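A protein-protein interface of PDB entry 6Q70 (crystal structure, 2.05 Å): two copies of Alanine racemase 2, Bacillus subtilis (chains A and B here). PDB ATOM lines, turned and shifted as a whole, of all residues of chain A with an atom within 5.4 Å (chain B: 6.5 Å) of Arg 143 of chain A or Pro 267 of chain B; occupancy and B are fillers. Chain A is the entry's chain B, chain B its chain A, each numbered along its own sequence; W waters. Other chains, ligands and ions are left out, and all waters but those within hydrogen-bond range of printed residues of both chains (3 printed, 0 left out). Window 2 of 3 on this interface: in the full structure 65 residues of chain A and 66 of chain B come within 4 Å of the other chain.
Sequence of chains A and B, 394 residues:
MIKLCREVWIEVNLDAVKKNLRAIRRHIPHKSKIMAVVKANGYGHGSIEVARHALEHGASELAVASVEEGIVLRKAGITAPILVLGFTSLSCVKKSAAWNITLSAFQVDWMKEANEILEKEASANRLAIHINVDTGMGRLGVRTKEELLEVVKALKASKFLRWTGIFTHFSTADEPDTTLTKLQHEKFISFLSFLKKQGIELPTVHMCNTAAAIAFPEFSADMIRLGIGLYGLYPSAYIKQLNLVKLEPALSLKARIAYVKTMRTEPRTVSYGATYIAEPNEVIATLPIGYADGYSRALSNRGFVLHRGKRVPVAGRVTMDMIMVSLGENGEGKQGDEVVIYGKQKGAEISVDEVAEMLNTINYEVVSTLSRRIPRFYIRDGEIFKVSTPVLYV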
ATOM      1  N   ASP A 134      26.868 -28.010  35.932  1.00  0.00           N
ATOM      2  CA  ASP A 134      25.584 -28.159  35.239  1.00  0.00           C
ATOM      3  C   ASP A 134      25.754 -29.457  34.529  1.00  0.00           C
ATOM      4  O   ASP A 134      26.581 -29.516  33.628  1.00  0.00           O
ATOM      5  CB  ASP A 134      25.377 -27.007  34.266  1.00  0.00           C
ATOM      6  CG  ASP A 134      24.139 -27.130  33.357  1.00  0.00           C
ATOM      7  OD1 ASP A 134      23.349 -28.083  33.506  1.00  0.00           O
ATOM      8  OD2 ASP A 134      23.925 -26.163  32.526  1.00  0.00           O
ATOM      9  N   THR A 135      25.016 -30.460  34.980  1.00  0.00           N
ATOM     10  CA  THR A 135      24.878 -31.820  34.325  1.00  0.00           C
ATOM     11  C   THR A 135      23.560 -32.015  33.605  1.00  0.00           C
ATOM     12  O   THR A 135      23.188 -33.142  33.186  1.00  0.00           O
ATOM     13  CB  THR A 135      25.016 -32.940  35.320  1.00  0.00           C
ATOM     14  OG1 THR A 135      24.025 -32.763  36.351  1.00  0.00           O
ATOM     15  CG2 THR A 135      26.389 -32.939  35.866  1.00  0.00           C
ATOM     16  N   GLY A 136      22.869 -30.924  33.318  1.00  0.00           N
ATOM     17  CA  GLY A 136      21.645 -31.052  32.515  1.00  0.00           C
ATOM     18  C   GLY A 136      20.485 -30.173  32.940  1.00  0.00           C
ATOM     19  O   GLY A 136      19.466 -30.090  32.170  1.00  0.00           O
ATOM     20  N   GLY A 138      20.741 -27.067  32.937  1.00  0.00           N
ATOM     21  CA  GLY A 138      20.836 -26.056  31.925  1.00  0.00           C
ATOM     22  C   GLY A 138      20.718 -24.601  32.525  1.00  0.00           C
ATOM     23  O   GLY A 138      20.553 -23.667  31.768  1.00  0.00           O
ATOM     24  N   GLY A 141      26.099 -23.125  36.052  1.00  0.00           N
ATOM     25  CA  GLY A 141      27.158 -24.086  36.326  1.00  0.00           C
ATOM     26  C   GLY A 141      28.016 -24.357  35.092  1.00  0.00           C
ATOM     27  O   GLY A 141      27.586 -24.051  33.987  1.00  0.00           O
ATOM     28  N   VAL A 142      29.224 -24.886  35.318  1.00  0.00           N
ATOM     29  CA  VAL A 142      30.151 -25.214  34.251  1.00  0.00           C
ATOM     30  C   VAL A 142      29.755 -26.558  33.587  1.00  0.00           C
ATOM     31  O   VAL A 142      29.250 -27.459  34.260  1.00  0.00           O
ATOM     32  CB  VAL A 142      31.577 -25.233  34.812  1.00  0.00           C
ATOM     33  CG1 VAL A 142      31.790 -26.290  35.916  1.00  0.00           C
ATOM     34  CG2 VAL A 142      32.589 -25.430  33.690  1.00  0.00           C
ATOM     35  N   ARG A 143      30.022 -26.728  32.287  1.00  0.00           N
ATOM     36  CA  ARG A 143      29.447 -27.854  31.507  1.00  0.00           C
ATOM     37  C   ARG A 143      30.405 -28.925  30.902  1.00  0.00           C
ATOM     38  O   ARG A 143      29.915 -29.925  30.415  1.00  0.00           O
ATOM     39  CB  ARG A 143      28.517 -27.325  30.409  1.00  0.00           C
ATOM     40  CG  ARG A 143      27.244 -26.709  30.992  1.00  0.00           C
ATOM     41  CD  ARG A 143      26.410 -26.046  29.933  1.00  0.00           C
ATOM     42  NE  ARG A 143      25.918 -26.990  28.916  1.00  0.00           N
ATOM     43  CZ  ARG A 143      24.727 -27.579  28.892  1.00  0.00           C
ATOM     44  NH1 ARG A 143      23.866 -27.407  29.924  1.00  0.00           N
ATOM     45  NH2 ARG A 143      24.374 -28.357  27.834  1.00  0.00           N
ATOM     46  N   THR A 144      31.707 -28.696  30.879  1.00  0.00           N
ATOM     47  CA  THR A 144      32.633 -29.703  30.358  1.00  0.00           C
ATOM     48  C   THR A 144      33.550 -29.975  31.463  1.00  0.00           C
ATOM     49  O   THR A 144      33.777 -29.068  32.304  1.00  0.00           O
ATOM     50  CB  THR A 144      33.501 -29.133  29.257  1.00  0.00           C
ATOM     51  OG1 THR A 144      34.298 -28.085  29.802  1.00  0.00           O
ATOM     52  CG2 THR A 144      32.673 -28.551  28.167  1.00  0.00           C
ATOM     53  N   LYS A 145      34.122 -31.165  31.486  1.00  0.00           N
ATOM     54  CA  LYS A 145      35.130 -31.457  32.526  1.00  0.00           C
ATOM     55  C   LYS A 145      36.430 -30.591  32.417  1.00  0.00           C
ATOM     56  O   LYS A 145      37.071 -30.258  33.463  1.00  0.00           O
ATOM     57  CB  LYS A 145      35.452 -32.940  32.547  1.00  0.00           C
ATOM     58  CG  LYS A 145      36.305 -33.372  31.360  1.00  0.00           C
ATOM     59  CD  LYS A 145      36.015 -34.809  30.999  1.00  0.00           C
ATOM     60  CE  LYS A 145      34.750 -34.823  30.164  1.00  0.00           C
ATOM     61  NZ  LYS A 145      34.408 -36.235  29.961  1.00  0.00           N
ATOM     62  N   LEU A 180      17.101 -39.772  32.584  1.00  0.00           N
ATOM     63  CA  LEU A 180      17.873 -38.537  32.660  1.00  0.00           C
ATOM     64  C   LEU A 180      18.616 -38.376  34.018  1.00  0.00           C
ATOM     65  O   LEU A 180      19.726 -37.814  34.053  1.00  0.00           O
ATOM     66  CB  LEU A 180      16.978 -37.311  32.492  1.00  0.00           C
ATOM     67  CG  LEU A 180      16.385 -37.029  31.097  1.00  0.00           C
ATOM     68  CD1 LEU A 180      17.490 -36.946  30.048  1.00  0.00           C
ATOM     69  CD2 LEU A 180      15.323 -38.092  30.715  1.00  0.00           C
ATOM     70  N   LYS A 187      27.248 -38.483  34.781  1.00  0.00           N
ATOM     71  CA  LYS A 187      28.089 -37.393  34.319  1.00  0.00           C
ATOM     72  C   LYS A 187      28.752 -36.702  35.519  1.00  0.00           C
ATOM     73  O   LYS A 187      29.932 -36.510  35.535  1.00  0.00           O
ATOM     74  CB  LYS A 187      27.249 -36.442  33.486  1.00  0.00           C
ATOM     75  CG  LYS A 187      27.983 -35.281  32.854  1.00  0.00           C
ATOM     76  CD  LYS A 187      27.178 -34.749  31.699  1.00  0.00           C
ATOM     77  CE  LYS A 187      28.050 -33.780  30.930  1.00  0.00           C
ATOM     78  NZ  LYS A 187      27.472 -33.397  29.609  1.00  0.00           N
ATOM     79  N   PHE A 191      32.819 -36.287  36.087  1.00  0.00           N
ATOM     80  CA  PHE A 191      33.579 -35.062  36.252  1.00  0.00           C
ATOM     81  C   PHE A 191      34.377 -35.098  37.555  1.00  0.00           C
ATOM     82  O   PHE A 191      35.519 -34.679  37.653  1.00  0.00           O
ATOM     83  CB  PHE A 191      32.656 -33.855  36.316  1.00  0.00           C
ATOM     84  CG  PHE A 191      32.121 -33.383  35.013  1.00  0.00           C
ATOM     85  CD1 PHE A 191      32.162 -34.161  33.832  1.00  0.00           C
ATOM     86  CD2 PHE A 191      31.599 -32.077  34.939  1.00  0.00           C
ATOM     87  CE1 PHE A 191      31.705 -33.637  32.645  1.00  0.00           C
ATOM     88  CE2 PHE A 191      31.134 -31.547  33.751  1.00  0.00           C
ATOM     89  CZ  PHE A 191      31.153 -32.342  32.608  1.00  0.00           C
ATOM     90  N   TYR B 259      24.006 -15.245  33.598  1.00  0.00           N
ATOM     91  CA  TYR B 259      24.868 -16.096  32.835  1.00  0.00           C
ATOM     92  C   TYR B 259      24.309 -16.327  31.481  1.00  0.00           C
ATOM     93  O   TYR B 259      23.115 -16.464  31.328  1.00  0.00           O
ATOM     94  CB  TYR B 259      24.977 -17.498  33.501  1.00  0.00           C
ATOM     95  CG  TYR B 259      25.989 -18.415  32.869  1.00  0.00           C
ATOM     96  CD1 TYR B 259      27.312 -17.974  32.629  1.00  0.00           C
ATOM     97  CD2 TYR B 259      25.667 -19.745  32.571  1.00  0.00           C
ATOM     98  CE1 TYR B 259      28.267 -18.839  32.099  1.00  0.00           C
ATOM     99  CE2 TYR B 259      26.628 -20.611  32.041  1.00  0.00           C
ATOM    100  CZ  TYR B 259      27.917 -20.151  31.813  1.00  0.00           C
ATOM    101  OH  TYR B 259      28.865 -20.972  31.274  1.00  0.00           O
ATOM    102  N   LYS B 261      25.318 -18.644  27.886  1.00  0.00           N
ATOM    103  CA  LYS B 261      26.062 -19.888  27.467  1.00  0.00           C
ATOM    104  C   LYS B 261      25.499 -20.323  26.147  1.00  0.00           C
ATOM    105  O   LYS B 261      24.317 -20.020  25.839  1.00  0.00           O
ATOM    106  CB  LYS B 261      25.913 -21.050  28.463  1.00  0.00           C
ATOM    107  CG  LYS B 261      24.486 -21.443  28.912  1.00  0.00           C
ATOM    108  CD  LYS B 261      24.501 -22.824  29.553  1.00  0.00           C
ATOM    109  CE  LYS B 261      23.201 -23.247  30.256  1.00  0.00           C
ATOM    110  NZ  LYS B 261      22.837 -22.425  31.466  1.00  0.00           N
ATOM    111  N   THR B 262      26.318 -20.995  25.358  1.00  0.00           N
ATOM    112  CA  THR B 262      25.854 -21.632  24.141  1.00  0.00           C
ATOM    113  C   THR B 262      25.695 -23.139  24.369  1.00  0.00           C
ATOM    114  O   THR B 262      26.584 -23.764  24.958  1.00  0.00           O
ATOM    115  CB  THR B 262      26.896 -21.350  23.038  1.00  0.00           C
ATOM    116  OG1 THR B 262      27.122 -19.940  23.032  1.00  0.00           O
ATOM    117  CG2 THR B 262      26.405 -21.798  21.647  1.00  0.00           C
ATOM    118  N   MET B 263      24.597 -23.748  23.908  1.00  0.00           N
ATOM    119  CA  MET B 263      24.322 -25.148  24.328  1.00  0.00           C
ATOM    120  C   MET B 263      25.034 -26.226  23.503  1.00  0.00           C
ATOM    121  O   MET B 263      24.401 -27.082  22.917  1.00  0.00           O
ATOM    122  CB  MET B 263      22.820 -25.443  24.383  1.00  0.00           C
ATOM    123  CG  MET B 263      21.993 -24.565  25.330  1.00  0.00           C
ATOM    124  SD  MET B 263      22.310 -24.814  27.041  1.00  0.00           S
ATOM    125  CE  MET B 263      21.656 -26.450  27.416  1.00  0.00           C
ATOM    126  N   ARG B 264      26.350 -26.233  23.547  1.00  0.00           N
ATOM    127  CA  ARG B 264      27.174 -27.121  22.681  1.00  0.00           C
ATOM    128  C   ARG B 264      27.194 -28.582  23.003  1.00  0.00           C
ATOM    129  O   ARG B 264      27.199 -29.388  22.090  1.00  0.00           O
ATOM    130  CB  ARG B 264      28.620 -26.704  22.720  1.00  0.00           C
ATOM    131  CG  ARG B 264      28.932 -25.820  21.555  1.00  0.00           C
ATOM    132  CD  ARG B 264      29.555 -24.568  22.059  1.00  0.00           C
ATOM    133  NE  ARG B 264      29.869 -23.665  20.968  1.00  0.00           N
ATOM    134  CZ  ARG B 264      30.489 -22.513  21.157  1.00  0.00           C
ATOM    135  NH1 ARG B 264      30.843 -22.132  22.396  1.00  0.00           N
ATOM    136  NH2 ARG B 264      30.746 -21.740  20.115  1.00  0.00           N
ATOM    137  N   THR B 265      27.219 -28.929  24.292  1.00  0.00           N
ATOM    138  CA  THR B 265      27.363 -30.304  24.726  1.00  0.00           C
ATOM    139  C   THR B 265      26.070 -30.869  25.265  1.00  0.00           C
ATOM    140  O   THR B 265      25.213 -30.101  25.769  1.00  0.00           O
ATOM    141  CB  THR B 265      28.482 -30.382  25.781  1.00  0.00           C
ATOM    142  OG1 THR B 265      28.188 -29.510  26.895  1.00  0.00           O
ATOM    143  CG2 THR B 265      29.838 -29.977  25.106  1.00  0.00           C
ATOM    144  N   GLU B 266      25.935 -32.199  25.187  1.00  0.00           N
ATOM    145  CA  GLU B 266      24.746 -32.918  25.648  1.00  0.00           C
ATOM    146  C   GLU B 266      24.799 -33.180  27.106  1.00  0.00           C
ATOM    147  O   GLU B 266      25.866 -33.273  27.605  1.00  0.00           O
ATOM    148  CB  GLU B 266      24.611 -34.232  24.971  1.00  0.00           C
ATOM    149  CG  GLU B 266      23.922 -34.062  23.649  1.00  0.00           C
ATOM    150  CD  GLU B 266      24.285 -35.193  22.722  1.00  0.00           C
ATOM    151  OE1 GLU B 266      24.509 -34.928  21.500  1.00  0.00           O
ATOM    152  OE2 GLU B 266      24.388 -36.341  23.257  1.00  0.00           O
ATOM    153  N   PRO B 267      23.662 -33.289  27.799  1.00  0.00           N
ATOM    154  CA  PRO B 267      22.330 -33.106  27.240  1.00  0.00           C
ATOM    155  C   PRO B 267      21.969 -31.616  27.120  1.00  0.00           C
ATOM    156  O   PRO B 267      22.508 -30.821  27.832  1.00  0.00           O
ATOM    157  CB  PRO B 267      21.423 -33.762  28.288  1.00  0.00           C
ATOM    158  CG  PRO B 267      22.143 -33.531  29.524  1.00  0.00           C
ATOM    159  CD  PRO B 267      23.559 -33.947  29.096  1.00  0.00           C
ATOM    160  N   ARG B 268      21.041 -31.268  26.254  1.00  0.00           N
ATOM    161  CA  ARG B 268      20.705 -29.861  26.001  1.00  0.00           C
ATOM    162  C   ARG B 268      19.376 -29.459  26.666  1.00  0.00           C
ATOM    163  O   ARG B 268      18.692 -28.502  26.265  1.00  0.00           O
ATOM    164  CB  ARG B 268      20.662 -29.561  24.501  1.00  0.00           C
ATOM    165  CG  ARG B 268      22.006 -29.809  23.844  1.00  0.00           C
ATOM    166  CD  ARG B 268      22.156 -29.294  22.403  1.00  0.00           C
ATOM    167  NE  ARG B 268      23.520 -29.686  22.034  1.00  0.00           N
ATOM    168  CZ  ARG B 268      23.877 -30.846  21.452  1.00  0.00           C
ATOM    169  NH1 ARG B 268      22.990 -31.738  21.062  1.00  0.00           N
ATOM    170  NH2 ARG B 268      25.144 -31.127  21.254  1.00  0.00           N
ATOM    171  N   THR B 269      19.037 -30.200  27.695  1.00  0.00           N
ATOM    172  CA  THR B 269      17.811 -29.985  28.430  1.00  0.00           C
ATOM    173  C   THR B 269      17.875 -28.697  29.283  1.00  0.00           C
ATOM    174  O   THR B 269      18.879 -28.375  29.896  1.00  0.00           O
ATOM    175  CB  THR B 269      17.581 -31.220  29.306  1.00  0.00           C
ATOM    176  OG1 THR B 269      18.751 -31.409  30.137  1.00  0.00           O
ATOM    177  CG2 THR B 269      17.313 -32.480  28.378  1.00  0.00           C
HETATM  178  O   HOH W   1      27.806 -27.018  26.550  1.00  0.00           O
HETATM  179  O   HOH W   2      16.695 -30.213  32.379  1.00  0.00           O
HETATM  180  O   HOH W   3      24.950 -23.759  33.140  1.00  0.00           O
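No position is printed for both chains.
Of the 12 pairs that touch across the chains among the printed residues, none has its exchanged pair printed and touching as well.
NZ of Lys 261 of chain B is in hydrogen-bond range of O of Gly 138 of chain A.
NH2 of Arg 143 of chain A is in hydrogen-bond range of O of Thr 265 of chain B (2.8 Å).
NZ of Lys 187 of chain A is in hydrogen-bond range of O of Glu 266 of chain B, 2.6 Å away.
The guanidinium group (NH2) of Arg 143 of chain A is in hydrogen-bond range of the backbone carbonyl oxygen (O) of Pro 267 of chain B (3.1 Å).
The side-chain hydroxyl of Thr 269 of chain B is in hydrogen-bond range of the backbone carbonyl oxygen of Gly 136 of chain A, 2.5 Å away.
The backbone carbonyl oxygen (O) of Met 263 of chain B lies within hydrogen-bond range of the guanidinium group (NE) of Arg 268 of chain B (2.9 Å).
The guanidinium group (NH1) of Arg 268 of chain B is in salt-bridge range of the side-chain carboxylate (OE1) of Glu 266 of chain B.
The backbone NH (N) of Gly 136 of chain A is in hydrogen-bond range of the side-chain carboxylate (OD1) of Asp 134 of chain A (2.9 Å).
OD1 of Asp 134 of chain A is in hydrogen-bond range of N of Gly 138 of chain A, at 2.9 Å.
N of Asp 134 of chain A is in hydrogen-bond range of O of Val 142 of chain A (3.0 Å).
OD2 of Asp 134 of chain A lies within salt-bridge range of NH1 of Arg 143 of chain A, 2.9 Å away.
Of the 12 printed residues of chain A, 6 touch a printed residue of chain B.
Of the 10 printed residues of chain B, 6 touch a printed residue of chain A.
Hydrophobic or aromatic side chains of chain B within 4 Å of the printed part of chain A: Met 263 and Pro 267.
Among the printed residues, no Asp or Glu carboxylate lies within 4 Å of a Lys or Arg side-chain nitrogen of the other chain.
Lys 261 of chain B touches Asp 134 of chain A (CE to OD2, 3.8 Å).
O of Thr 135 of chain A touches CG of Pro 267 of chain B (3.8 Å).
Gly 136 of chain A touches Pro 267 of chain B (CA to CG, 3.9 Å).
CA of Gly 138 of chain A touches O of Thr 269 of chain B, at 3.7 Å.
Arg 143 of chain A touches Lys 261 of chain B.
CE of Met 263 of chain B touches NH2 of Arg 143 of chain A (3.3 Å).
NZ of Lys 187 of chain A touches CD of Pro 267 of chain B, 3.98 Å away.
Of the printed residues of chain B, Arg 143 of chain A touches Lys 261, Met 263, Thr 265 and Pro 267.
Of the printed residues of chain A, Pro 267 of chain B touches Thr 135, Gly 136, Arg 143 and Lys 187.
Of the printed residues of chain B, Gly 136 of chain A touches Pro 267 and Thr 269.
Of the printed residues of chain A, Thr 269 of chain B touches Gly 136 (2.5 Å) and Gly 138 (3.7 Å).
Gly 141 of chain A touches none of the printed residues of chain B.
The nearest residue of chain B that does not touch Arg 143 of chain A is Arg 268 of chain B (4.4 Å).
The nearest printed residue of chain A that does not touch Pro 267 of chain B is Leu 180 of chain A (5.4 Å).
Water W1 lies within hydrogen-bond range of the side-chain hydroxyl of Thr 265 of chain B, the guanidinium group of Arg 143 of chain A and the backbone NH of Arg 264 of chain B.
Water W3 lies within hydrogen-bond range of the side-chain carboxylate of Asp 134 of chain A (2.7 Å), the backbone carbonyl oxygen of Gly 141 of chain A (2.8 Å) and the side-chain amino group of Lys 261 of chain B (3.0 Å).
Water W2 lies within hydrogen-bond range of O of Gly 136 of chain A and OG1 of Thr 269 of chain B.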
